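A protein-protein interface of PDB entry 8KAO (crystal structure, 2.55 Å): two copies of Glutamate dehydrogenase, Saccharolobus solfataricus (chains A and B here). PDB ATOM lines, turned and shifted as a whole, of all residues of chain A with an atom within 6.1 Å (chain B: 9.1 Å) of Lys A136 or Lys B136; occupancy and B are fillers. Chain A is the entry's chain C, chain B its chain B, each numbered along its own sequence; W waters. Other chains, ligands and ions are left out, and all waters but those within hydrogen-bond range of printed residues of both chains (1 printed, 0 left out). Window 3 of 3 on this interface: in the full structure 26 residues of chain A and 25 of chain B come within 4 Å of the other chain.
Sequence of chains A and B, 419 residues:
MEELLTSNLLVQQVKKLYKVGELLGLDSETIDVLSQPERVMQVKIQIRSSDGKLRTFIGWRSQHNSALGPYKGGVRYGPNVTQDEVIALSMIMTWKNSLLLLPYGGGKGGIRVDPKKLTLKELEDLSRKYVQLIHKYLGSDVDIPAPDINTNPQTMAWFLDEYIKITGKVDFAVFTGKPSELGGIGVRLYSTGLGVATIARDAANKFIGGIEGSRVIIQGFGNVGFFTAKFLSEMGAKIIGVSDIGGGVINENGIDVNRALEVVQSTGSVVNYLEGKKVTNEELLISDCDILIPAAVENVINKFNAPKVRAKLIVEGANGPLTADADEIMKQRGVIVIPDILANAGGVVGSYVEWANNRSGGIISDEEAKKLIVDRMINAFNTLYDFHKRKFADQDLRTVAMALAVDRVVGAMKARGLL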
ATOM      1  N   VAL A 131      -4.312  -6.161 -39.270  1.00  0.00           N
ATOM      2  CA  VAL A 131      -3.886  -7.540 -39.139  1.00  0.00           C
ATOM      3  C   VAL A 131      -2.770  -7.626 -38.103  1.00  0.00           C
ATOM      4  O   VAL A 131      -2.833  -8.411 -37.158  1.00  0.00           O
ATOM      5  CB  VAL A 131      -3.478  -8.102 -40.515  1.00  0.00           C
ATOM      6  CG1 VAL A 131      -2.588  -9.324 -40.388  1.00  0.00           C
ATOM      7  CG2 VAL A 131      -4.703  -8.412 -41.373  1.00  0.00           C
ATOM      8  N   GLN A 132      -1.750  -6.788 -38.246  1.00  0.00           N
ATOM      9  CA  GLN A 132      -0.573  -6.910 -37.399  1.00  0.00           C
ATOM     10  C   GLN A 132      -0.945  -6.748 -35.918  1.00  0.00           C
ATOM     11  O   GLN A 132      -0.310  -7.364 -35.053  1.00  0.00           O
ATOM     12  CB  GLN A 132       0.495  -5.919 -37.858  1.00  0.00           C
ATOM     13  CG  GLN A 132       1.822  -6.052 -37.116  1.00  0.00           C
ATOM     14  CD  GLN A 132       1.852  -5.356 -35.773  1.00  0.00           C
ATOM     15  OE1 GLN A 132       1.363  -4.235 -35.631  1.00  0.00           O
ATOM     16  NE2 GLN A 132       2.430  -6.016 -34.777  1.00  0.00           N
ATOM     17  N   LEU A 133      -1.966  -5.931 -35.614  1.00  0.00           N
ATOM     18  CA  LEU A 133      -2.296  -5.620 -34.223  1.00  0.00           C
ATOM     19  C   LEU A 133      -3.185  -6.703 -33.581  1.00  0.00           C
ATOM     20  O   LEU A 133      -3.393  -6.704 -32.364  1.00  0.00           O
ATOM     21  CB  LEU A 133      -2.946  -4.228 -34.194  1.00  0.00           C
ATOM     22  CG  LEU A 133      -1.986  -3.034 -34.317  1.00  0.00           C
ATOM     23  CD1 LEU A 133      -2.721  -1.760 -34.705  1.00  0.00           C
ATOM     24  CD2 LEU A 133      -1.267  -2.800 -33.004  1.00  0.00           C
ATOM     25  N   ILE A 134      -3.715  -7.643 -34.384  1.00  0.00           N
ATOM     26  CA  ILE A 134      -4.562  -8.710 -33.864  1.00  0.00           C
ATOM     27  C   ILE A 134      -4.020 -10.103 -34.209  1.00  0.00           C
ATOM     28  O   ILE A 134      -4.640 -11.094 -33.825  1.00  0.00           O
ATOM     29  CB  ILE A 134      -6.011  -8.563 -34.378  1.00  0.00           C
ATOM     30  CG1 ILE A 134      -6.112  -8.682 -35.896  1.00  0.00           C
ATOM     31  CG2 ILE A 134      -6.657  -7.277 -33.888  1.00  0.00           C
ATOM     32  CD1 ILE A 134      -7.526  -8.541 -36.410  1.00  0.00           C
ATOM     33  N   HIS A 135      -2.868 -10.187 -34.898  1.00  0.00           N
ATOM     34  CA  HIS A 135      -2.479 -11.401 -35.614  1.00  0.00           C
ATOM     35  C   HIS A 135      -2.264 -12.590 -34.679  1.00  0.00           C
ATOM     36  O   HIS A 135      -2.202 -13.735 -35.134  1.00  0.00           O
ATOM     37  CB  HIS A 135      -1.185 -11.203 -36.415  1.00  0.00           C
ATOM     38  CG  HIS A 135       0.081 -11.258 -35.626  1.00  0.00           C
ATOM     39  ND1 HIS A 135       0.636 -10.136 -35.042  1.00  0.00           N
ATOM     40  CD2 HIS A 135       0.892 -12.285 -35.307  1.00  0.00           C
ATOM     41  CE1 HIS A 135       1.773 -10.475 -34.417  1.00  0.00           C
ATOM     42  NE2 HIS A 135       1.946 -11.779 -34.560  1.00  0.00           N
ATOM     43  N   LYS A 136      -2.118 -12.339 -33.374  1.00  0.00           N
ATOM     44  CA  LYS A 136      -1.940 -13.449 -32.458  1.00  0.00           C
ATOM     45  C   LYS A 136      -3.263 -14.169 -32.236  1.00  0.00           C
ATOM     46  O   LYS A 136      -3.247 -15.277 -31.695  1.00  0.00           O
ATOM     47  CB  LYS A 136      -1.418 -13.005 -31.094  1.00  0.00           C
ATOM     48  CG  LYS A 136      -0.036 -12.392 -31.113  1.00  0.00           C
ATOM     49  CD  LYS A 136       1.085 -13.391 -31.229  1.00  0.00           C
ATOM     50  CE  LYS A 136       2.407 -12.659 -31.343  1.00  0.00           C
ATOM     51  NZ  LYS A 136       3.552 -13.520 -31.003  1.00  0.00           N
ATOM     52  N   TYR A 137      -4.394 -13.506 -32.541  1.00  0.00           N
ATOM     53  CA  TYR A 137      -5.675 -14.188 -32.425  1.00  0.00           C
ATOM     54  C   TYR A 137      -6.300 -14.383 -33.801  1.00  0.00           C
ATOM     55  O   TYR A 137      -7.516 -14.541 -33.881  1.00  0.00           O
ATOM     56  CB  TYR A 137      -6.591 -13.510 -31.412  1.00  0.00           C
ATOM     57  CG  TYR A 137      -6.369 -13.950 -29.982  1.00  0.00           C
ATOM     58  CD1 TYR A 137      -6.631 -15.252 -29.565  1.00  0.00           C
ATOM     59  CD2 TYR A 137      -5.914 -13.041 -29.035  1.00  0.00           C
ATOM     60  CE1 TYR A 137      -6.417 -15.635 -28.245  1.00  0.00           C
ATOM     61  CE2 TYR A 137      -5.720 -13.400 -27.715  1.00  0.00           C
ATOM     62  CZ  TYR A 137      -5.959 -14.706 -27.313  1.00  0.00           C
ATOM     63  OH  TYR A 137      -5.747 -14.990 -25.970  1.00  0.00           O
ATOM     64  N   LEU A 138      -5.424 -14.488 -34.823  1.00  0.00           N
ATOM     65  CA  LEU A 138      -5.764 -14.947 -36.164  1.00  0.00           C
ATOM     66  C   LEU A 138      -5.024 -16.258 -36.445  1.00  0.00           C
ATOM     67  O   LEU A 138      -4.147 -16.660 -35.687  1.00  0.00           O
ATOM     68  CB  LEU A 138      -5.347 -13.902 -37.202  1.00  0.00           C
ATOM     69  CG  LEU A 138      -5.952 -12.509 -37.077  1.00  0.00           C
ATOM     70  CD1 LEU A 138      -5.488 -11.654 -38.250  1.00  0.00           C
ATOM     71  CD2 LEU A 138      -7.480 -12.564 -37.006  1.00  0.00           C
ATOM     72  N   VAL A 142      -7.829 -20.422 -36.343  1.00  0.00           N
ATOM     73  CA  VAL A 142      -8.214 -19.557 -35.236  1.00  0.00           C
ATOM     74  C   VAL A 142      -9.285 -18.564 -35.689  1.00  0.00           C
ATOM     75  O   VAL A 142     -10.386 -18.559 -35.123  1.00  0.00           O
ATOM     76  CB  VAL A 142      -7.002 -18.806 -34.666  1.00  0.00           C
ATOM     77  CG1 VAL A 142      -7.415 -17.901 -33.510  1.00  0.00           C
ATOM     78  CG2 VAL A 142      -5.895 -19.769 -34.268  1.00  0.00           C
ATOM     79  N   ARG B  39      -4.156  -1.693 -27.691  1.00  0.00           N
ATOM     80  CA  ARG B  39      -5.075  -2.797 -27.813  1.00  0.00           C
ATOM     81  C   ARG B  39      -5.901  -2.889 -26.540  1.00  0.00           C
ATOM     82  O   ARG B  39      -5.411  -2.570 -25.458  1.00  0.00           O
ATOM     83  CB  ARG B  39      -4.299  -4.084 -28.059  1.00  0.00           C
ATOM     84  CG  ARG B  39      -5.203  -5.337 -28.278  1.00  0.00           C
ATOM     85  CD  ARG B  39      -4.333  -6.549 -28.713  1.00  0.00           C
ATOM     86  NE  ARG B  39      -2.974  -6.381 -28.214  1.00  0.00           N
ATOM     87  CZ  ARG B  39      -1.925  -6.043 -28.967  1.00  0.00           C
ATOM     88  NH1 ARG B  39      -2.029  -6.051 -30.281  1.00  0.00           N
ATOM     89  NH2 ARG B  39      -0.759  -5.753 -28.398  1.00  0.00           N
ATOM     90  N   MET B  41      -8.840  -5.908 -25.029  1.00  0.00           N
ATOM     91  CA  MET B  41      -9.679  -7.060 -25.293  1.00  0.00           C
ATOM     92  C   MET B  41     -10.710  -7.242 -24.188  1.00  0.00           C
ATOM     93  O   MET B  41     -10.477  -6.925 -23.018  1.00  0.00           O
ATOM     94  CB  MET B  41      -8.877  -8.355 -25.464  1.00  0.00           C
ATOM     95  CG  MET B  41      -7.387  -8.173 -25.392  1.00  0.00           C
ATOM     96  SD  MET B  41      -6.510  -9.739 -25.488  1.00  0.00           S
ATOM     97  CE  MET B  41      -5.014  -9.226 -24.645  1.00  0.00           C
ATOM     98  N   GLN B  63      -4.392  -2.555 -22.861  1.00  0.00           N
ATOM     99  CA  GLN B  63      -2.975  -2.484 -23.110  1.00  0.00           C
ATOM    100  C   GLN B  63      -2.759  -1.115 -23.740  1.00  0.00           C
ATOM    101  O   GLN B  63      -2.921  -0.953 -24.947  1.00  0.00           O
ATOM    102  CB  GLN B  63      -2.592  -3.667 -24.001  1.00  0.00           C
ATOM    103  CG  GLN B  63      -2.938  -5.011 -23.374  1.00  0.00           C
ATOM    104  CD  GLN B  63      -2.559  -6.253 -24.151  1.00  0.00           C
ATOM    105  OE1 GLN B  63      -2.583  -6.283 -25.380  1.00  0.00           O
ATOM    106  NE2 GLN B  63      -2.261  -7.325 -23.421  1.00  0.00           N
ATOM    107  N   TYR B  71       3.396  -4.028 -21.487  1.00  0.00           N
ATOM    108  CA  TYR B  71       2.335  -3.539 -20.631  1.00  0.00           C
ATOM    109  C   TYR B  71       2.529  -4.133 -19.239  1.00  0.00           C
ATOM    110  O   TYR B  71       2.835  -5.316 -19.144  1.00  0.00           O
ATOM    111  CB  TYR B  71       0.976  -3.915 -21.233  1.00  0.00           C
ATOM    112  CG  TYR B  71       0.837  -3.660 -22.715  1.00  0.00           C
ATOM    113  CD1 TYR B  71       0.781  -2.375 -23.215  1.00  0.00           C
ATOM    114  CD2 TYR B  71       0.795  -4.704 -23.618  1.00  0.00           C
ATOM    115  CE1 TYR B  71       0.660  -2.133 -24.570  1.00  0.00           C
ATOM    116  CE2 TYR B  71       0.657  -4.483 -24.977  1.00  0.00           C
ATOM    117  CZ  TYR B  71       0.584  -3.191 -25.453  1.00  0.00           C
ATOM    118  OH  TYR B  71       0.453  -2.960 -26.795  1.00  0.00           O
ATOM    119  N   TYR B 130     -10.130 -16.008 -17.280  1.00  0.00           N
ATOM    120  CA  TYR B 130      -9.735 -14.686 -17.746  1.00  0.00           C
ATOM    121  C   TYR B 130      -8.364 -14.769 -18.418  1.00  0.00           C
ATOM    122  O   TYR B 130      -8.200 -14.440 -19.592  1.00  0.00           O
ATOM    123  CB  TYR B 130      -9.729 -13.714 -16.560  1.00  0.00           C
ATOM    124  CG  TYR B 130      -9.181 -12.333 -16.839  1.00  0.00           C
ATOM    125  CD1 TYR B 130      -9.947 -11.366 -17.476  1.00  0.00           C
ATOM    126  CD2 TYR B 130      -7.886 -11.990 -16.475  1.00  0.00           C
ATOM    127  CE1 TYR B 130      -9.443 -10.100 -17.750  1.00  0.00           C
ATOM    128  CE2 TYR B 130      -7.364 -10.730 -16.741  1.00  0.00           C
ATOM    129  CZ  TYR B 130      -8.150  -9.778 -17.372  1.00  0.00           C
ATOM    130  OH  TYR B 130      -7.663  -8.523 -17.627  1.00  0.00           O
ATOM    131  N   VAL B 131      -7.376 -15.239 -17.653  1.00  0.00           N
ATOM    132  CA  VAL B 131      -6.035 -15.471 -18.158  1.00  0.00           C
ATOM    133  C   VAL B 131      -6.067 -16.252 -19.473  1.00  0.00           C
ATOM    134  O   VAL B 131      -5.442 -15.863 -20.466  1.00  0.00           O
ATOM    135  CB  VAL B 131      -5.235 -16.201 -17.073  1.00  0.00           C
ATOM    136  CG1 VAL B 131      -4.111 -17.033 -17.655  1.00  0.00           C
ATOM    137  CG2 VAL B 131      -4.735 -15.209 -16.028  1.00  0.00           C
ATOM    138  N   GLN B 132      -6.827 -17.346 -19.469  1.00  0.00           N
ATOM    139  CA  GLN B 132      -6.882 -18.282 -20.584  1.00  0.00           C
ATOM    140  C   GLN B 132      -7.373 -17.598 -21.854  1.00  0.00           C
ATOM    141  O   GLN B 132      -6.863 -17.852 -22.939  1.00  0.00           O
ATOM    142  CB  GLN B 132      -7.816 -19.438 -20.225  1.00  0.00           C
ATOM    143  CG  GLN B 132      -7.761 -20.599 -21.208  1.00  0.00           C
ATOM    144  CD  GLN B 132      -8.676 -20.399 -22.394  1.00  0.00           C
ATOM    145  OE1 GLN B 132      -9.867 -20.120 -22.222  1.00  0.00           O
ATOM    146  NE2 GLN B 132      -8.131 -20.570 -23.595  1.00  0.00           N
ATOM    147  N   LEU B 133      -8.382 -16.738 -21.701  1.00  0.00           N
ATOM    148  CA  LEU B 133      -9.037 -16.099 -22.829  1.00  0.00           C
ATOM    149  C   LEU B 133      -8.182 -14.960 -23.401  1.00  0.00           C
ATOM    150  O   LEU B 133      -8.455 -14.500 -24.507  1.00  0.00           O
ATOM    151  CB  LEU B 133     -10.418 -15.623 -22.355  1.00  0.00           C
ATOM    152  CG  LEU B 133     -11.476 -16.726 -22.206  1.00  0.00           C
ATOM    153  CD1 LEU B 133     -12.595 -16.308 -21.266  1.00  0.00           C
ATOM    154  CD2 LEU B 133     -12.072 -17.089 -23.563  1.00  0.00           C
ATOM    155  N   ILE B 134      -7.127 -14.522 -22.689  1.00  0.00           N
ATOM    156  CA  ILE B 134      -6.296 -13.422 -23.159  1.00  0.00           C
ATOM    157  C   ILE B 134      -4.816 -13.803 -23.280  1.00  0.00           C
ATOM    158  O   ILE B 134      -4.033 -12.915 -23.589  1.00  0.00           O
ATOM    159  CB  ILE B 134      -6.421 -12.195 -22.227  1.00  0.00           C
ATOM    160  CG1 ILE B 134      -5.760 -12.454 -20.873  1.00  0.00           C
ATOM    161  CG2 ILE B 134      -7.859 -11.734 -22.046  1.00  0.00           C
ATOM    162  CD1 ILE B 134      -5.665 -11.223 -19.996  1.00  0.00           C
ATOM    163  N   HIS B 135      -4.396 -15.059 -23.023  1.00  0.00           N
ATOM    164  CA  HIS B 135      -2.976 -15.334 -22.783  1.00  0.00           C
ATOM    165  C   HIS B 135      -2.130 -15.019 -24.014  1.00  0.00           C
ATOM    166  O   HIS B 135      -0.956 -14.662 -23.905  1.00  0.00           O
ATOM    167  CB  HIS B 135      -2.683 -16.769 -22.305  1.00  0.00           C
ATOM    168  CG  HIS B 135      -2.863 -17.823 -23.333  1.00  0.00           C
ATOM    169  ND1 HIS B 135      -4.117 -18.247 -23.711  1.00  0.00           N
ATOM    170  CD2 HIS B 135      -1.986 -18.527 -24.066  1.00  0.00           C
ATOM    171  CE1 HIS B 135      -4.005 -19.190 -24.661  1.00  0.00           C
ATOM    172  NE2 HIS B 135      -2.718 -19.353 -24.917  1.00  0.00           N
ATOM    173  N   LYS B 136      -2.717 -15.108 -25.203  1.00  0.00           N
ATOM    174  CA  LYS B 136      -1.923 -14.885 -26.399  1.00  0.00           C
ATOM    175  C   LYS B 136      -1.393 -13.449 -26.429  1.00  0.00           C
ATOM    176  O   LYS B 136      -0.504 -13.170 -27.225  1.00  0.00           O
ATOM    177  CB  LYS B 136      -2.746 -15.213 -27.642  1.00  0.00           C
ATOM    178  CG  LYS B 136      -3.256 -16.648 -27.724  1.00  0.00           C
ATOM    179  CD  LYS B 136      -2.142 -17.601 -28.072  1.00  0.00           C
ATOM    180  CE  LYS B 136      -2.595 -18.981 -28.499  1.00  0.00           C
ATOM    181  NZ  LYS B 136      -1.429 -19.890 -28.659  1.00  0.00           N
ATOM    182  N   TYR B 137      -1.913 -12.527 -25.600  1.00  0.00           N
ATOM    183  CA  TYR B 137      -1.272 -11.221 -25.425  1.00  0.00           C
ATOM    184  C   TYR B 137      -0.897 -10.983 -23.956  1.00  0.00           C
ATOM    185  O   TYR B 137      -0.995  -9.857 -23.458  1.00  0.00           O
ATOM    186  CB  TYR B 137      -2.163 -10.110 -25.981  1.00  0.00           C
ATOM    187  CG  TYR B 137      -2.215 -10.016 -27.490  1.00  0.00           C
ATOM    188  CD1 TYR B 137      -1.113  -9.594 -28.230  1.00  0.00           C
ATOM    189  CD2 TYR B 137      -3.394 -10.270 -28.181  1.00  0.00           C
ATOM    190  CE1 TYR B 137      -1.170  -9.498 -29.611  1.00  0.00           C
ATOM    191  CE2 TYR B 137      -3.467 -10.172 -29.562  1.00  0.00           C
ATOM    192  CZ  TYR B 137      -2.343  -9.800 -30.287  1.00  0.00           C
ATOM    193  OH  TYR B 137      -2.391  -9.673 -31.678  1.00  0.00           O
ATOM    194  N   LEU B 138      -0.453 -12.059 -23.277  1.00  0.00           N
ATOM    195  CA  LEU B 138       0.219 -11.962 -21.998  1.00  0.00           C
ATOM    196  C   LEU B 138       1.605 -12.571 -22.154  1.00  0.00           C
ATOM    197  O   LEU B 138       1.833 -13.403 -23.033  1.00  0.00           O
ATOM    198  CB  LEU B 138      -0.566 -12.727 -20.929  1.00  0.00           C
ATOM    199  CG  LEU B 138      -1.955 -12.202 -20.548  1.00  0.00           C
ATOM    200  CD1 LEU B 138      -2.529 -13.063 -19.445  1.00  0.00           C
ATOM    201  CD2 LEU B 138      -1.911 -10.762 -20.090  1.00  0.00           C
ATOM    202  N   GLY B 139       2.533 -12.150 -21.289  1.00  0.00           N
ATOM    203  CA  GLY B 139       3.816 -12.816 -21.187  1.00  0.00           C
ATOM    204  C   GLY B 139       4.775 -11.971 -20.375  1.00  0.00           C
ATOM    205  O   GLY B 139       4.462 -10.821 -20.109  1.00  0.00           O
ATOM    206  N   VAL B 142       5.574  -9.248 -22.737  1.00  0.00           N
ATOM    207  CA  VAL B 142       4.493  -8.625 -23.500  1.00  0.00           C
ATOM    208  C   VAL B 142       3.500  -7.898 -22.584  1.00  0.00           C
ATOM    209  O   VAL B 142       3.264  -6.705 -22.798  1.00  0.00           O
ATOM    210  CB  VAL B 142       3.825  -9.596 -24.503  1.00  0.00           C
ATOM    211  CG1 VAL B 142       4.423 -10.987 -24.467  1.00  0.00           C
ATOM    212  CG2 VAL B 142       2.312  -9.647 -24.370  1.00  0.00           C
ATOM    213  N   ASP B 143       2.907  -8.597 -21.597  1.00  0.00           N
ATOM    214  CA  ASP B 143       1.958  -7.993 -20.659  1.00  0.00           C
ATOM    215  C   ASP B 143       1.981  -8.767 -19.333  1.00  0.00           C
ATOM    216  O   ASP B 143       1.726  -9.969 -19.308  1.00  0.00           O
ATOM    217  CB  ASP B 143       0.531  -7.939 -21.230  1.00  0.00           C
ATOM    218  CG  ASP B 143      -0.433  -7.088 -20.409  1.00  0.00           C
ATOM    219  OD1 ASP B 143       0.042  -6.501 -19.415  1.00  0.00           O
ATOM    220  OD2 ASP B 143      -1.648  -6.968 -20.797  1.00  0.00           O
ATOM    221  N   TYR B 163      -1.597 -20.344 -16.407  1.00  0.00           N
ATOM    222  CA  TYR B 163      -0.627 -19.976 -17.421  1.00  0.00           C
ATOM    223  C   TYR B 163       0.317 -21.159 -17.642  1.00  0.00           C
ATOM    224  O   TYR B 163       0.543 -21.574 -18.785  1.00  0.00           O
ATOM    225  CB  TYR B 163       0.085 -18.687 -17.020  1.00  0.00           C
ATOM    226  CG  TYR B 163       0.907 -18.078 -18.124  1.00  0.00           C
ATOM    227  CD1 TYR B 163       0.339 -17.249 -19.083  1.00  0.00           C
ATOM    228  CD2 TYR B 163       2.252 -18.395 -18.252  1.00  0.00           C
ATOM    229  CE1 TYR B 163       1.093 -16.738 -20.130  1.00  0.00           C
ATOM    230  CE2 TYR B 163       3.017 -17.890 -19.291  1.00  0.00           C
ATOM    231  CZ  TYR B 163       2.442 -17.046 -20.225  1.00  0.00           C
ATOM    232  OH  TYR B 163       3.229 -16.530 -21.234  1.00  0.00           O
ATOM    233  N   ILE B 166      -1.286 -23.762 -19.746  1.00  0.00           N
ATOM    234  CA  ILE B 166      -1.458 -23.495 -21.163  1.00  0.00           C
ATOM    235  C   ILE B 166      -0.116 -23.574 -21.896  1.00  0.00           C
ATOM    236  O   ILE B 166       0.005 -24.267 -22.907  1.00  0.00           O
ATOM    237  CB  ILE B 166      -2.131 -22.121 -21.323  1.00  0.00           C
ATOM    238  CG1 ILE B 166      -3.527 -22.118 -20.695  1.00  0.00           C
ATOM    239  CG2 ILE B 166      -2.189 -21.717 -22.787  1.00  0.00           C
ATOM    240  CD1 ILE B 166      -3.978 -20.739 -20.279  1.00  0.00           C
ATOM    241  N   THR B 167       0.878 -22.818 -21.405  1.00  0.00           N
ATOM    242  CA  THR B 167       2.170 -22.699 -22.064  1.00  0.00           C
ATOM    243  C   THR B 167       3.067 -23.903 -21.755  1.00  0.00           C
ATOM    244  O   THR B 167       3.880 -24.311 -22.581  1.00  0.00           O
ATOM    245  CB  THR B 167       2.862 -21.397 -21.647  1.00  0.00           C
ATOM    246  OG1 THR B 167       3.186 -21.431 -20.252  1.00  0.00           O
ATOM    247  CG2 THR B 167       1.993 -20.196 -21.940  1.00  0.00           C
ATOM    248  N   LYS B 169       5.246 -23.742 -19.227  1.00  0.00           N
ATOM    249  CA  LYS B 169       6.487 -23.177 -18.726  1.00  0.00           C
ATOM    250  C   LYS B 169       6.224 -22.538 -17.364  1.00  0.00           C
ATOM    251  O   LYS B 169       5.210 -21.858 -17.168  1.00  0.00           O
ATOM    252  CB  LYS B 169       7.040 -22.097 -19.668  1.00  0.00           C
ATOM    253  CG  LYS B 169       7.133 -22.448 -21.153  1.00  0.00           C
ATOM    254  CD  LYS B 169       7.283 -21.181 -22.030  1.00  0.00           C
ATOM    255  CE  LYS B 169       7.328 -21.460 -23.522  1.00  0.00           C
ATOM    256  NZ  LYS B 169       5.969 -21.481 -24.128  1.00  0.00           N
HETATM  257  O   HOH W   1      -0.282  -8.184 -32.581  1.00  0.00           O
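OH of Tyr B137 lies within hydrogen-bond range of N of His A135.
The backbone NH of Lys A136 is in hydrogen-bond range of the side-chain hydroxyl of Tyr B137, at 3.2 Å.
The side-chain hydroxyl (OH) of Tyr A137 sits at hydrogen-bond distance from the backbone NH (N) of Lys B136 (3.1 Å).
The backbone NH (N) of His B135 is in hydrogen-bond range of the side-chain hydroxyl (OH) of Tyr A137, at 3.2 Å.
The guanidinium group (NH1) of Arg B39 sits at hydrogen-bond distance from the backbone carbonyl oxygen (O) of Leu A133.
The backbone carbonyl oxygen (O) of Leu B133 lies within hydrogen-bond range of the side-chain hydroxyl (OH) of Tyr A137.
OH of Tyr B137 is in hydrogen-bond range of O of Leu A133, at 3.2 Å.
The side-chain hydroxyl of Tyr B137 lies close to the backbone carbonyl oxygen of Ile A134 (3.4 Å).
O of Gln B132 lies within hydrogen-bond range of ND1 of His B135, 2.9 Å away.
O of Gln A132 sits at hydrogen-bond distance from ND1 of His A135.
The backbone carbonyl oxygen (O) of Tyr B137 is in hydrogen-bond range of the side-chain amide nitrogen (NE2) of Gln B63, 2.8 Å away.
NH2 of Arg B39 sits at hydrogen-bond distance from OH of Tyr B71 (3.4 Å).
The backbone carbonyl oxygen (O) of Arg B39 sits at hydrogen-bond distance from the backbone NH (N) of Gln B63 (2.8 Å).
Lys A136 touches Lys B136.
Ile B134 touches Tyr A137.
Tyr A137 touches Tyr B137 (CD2 to CE2, 3.8 Å).
Printed residues of chain B within 4 Å of Leu A133: Arg B39 (2.6 Å) and Tyr B137 (3.2 Å).
Of the printed residues of chain A, Ile B134 touches Tyr A137 (3.1 Å).
Lys B136 touches just these residues of chain A: Lys A136 (3.98 Å) and Tyr A137 (3.1 Å).
The nearest printed residue of chain A that does not touch Lys B136 is Val A142 (6.7 Å).
Of the 9 printed residues of chain A, 5 touch a printed residue of chain B.
Printed residues of chain A that touch a printed residue of chain B: Leu A133, Ile A134, His A135, Lys A136 and Tyr A137.
Hydrophobic or aromatic side chains of chain A that line the printed part of chain B: Tyr A137.
Among the printed residues, 11 pairs touch across the chains.
Among the printed residues, no Asp or Glu carboxylate lies within 4 Å of a Lys or Arg side-chain nitrogen of the other chain.
Leu A133 touches Tyr B137, and with the chains exchanged Tyr A137 touches Leu B133.
Ile A134 touches Tyr B137, and with the chains exchanged Tyr A137 touches Ile B134.
His A135 touches Tyr B137, and with the chains exchanged Tyr A137 touches His B135.
Tyr A137 touches its own counterpart, Tyr B137.
Positions printed for both chains: 131, 132, 133, 134, 135, 136, 137, 138 and 142.
Water W1 lies within hydrogen-bond range of O of Gln A132 (2.6 Å), OH of Tyr B137 (2.7 Å), ND1 of His A135 (3.3 Å) and O of Leu A133 (3.5 Å).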
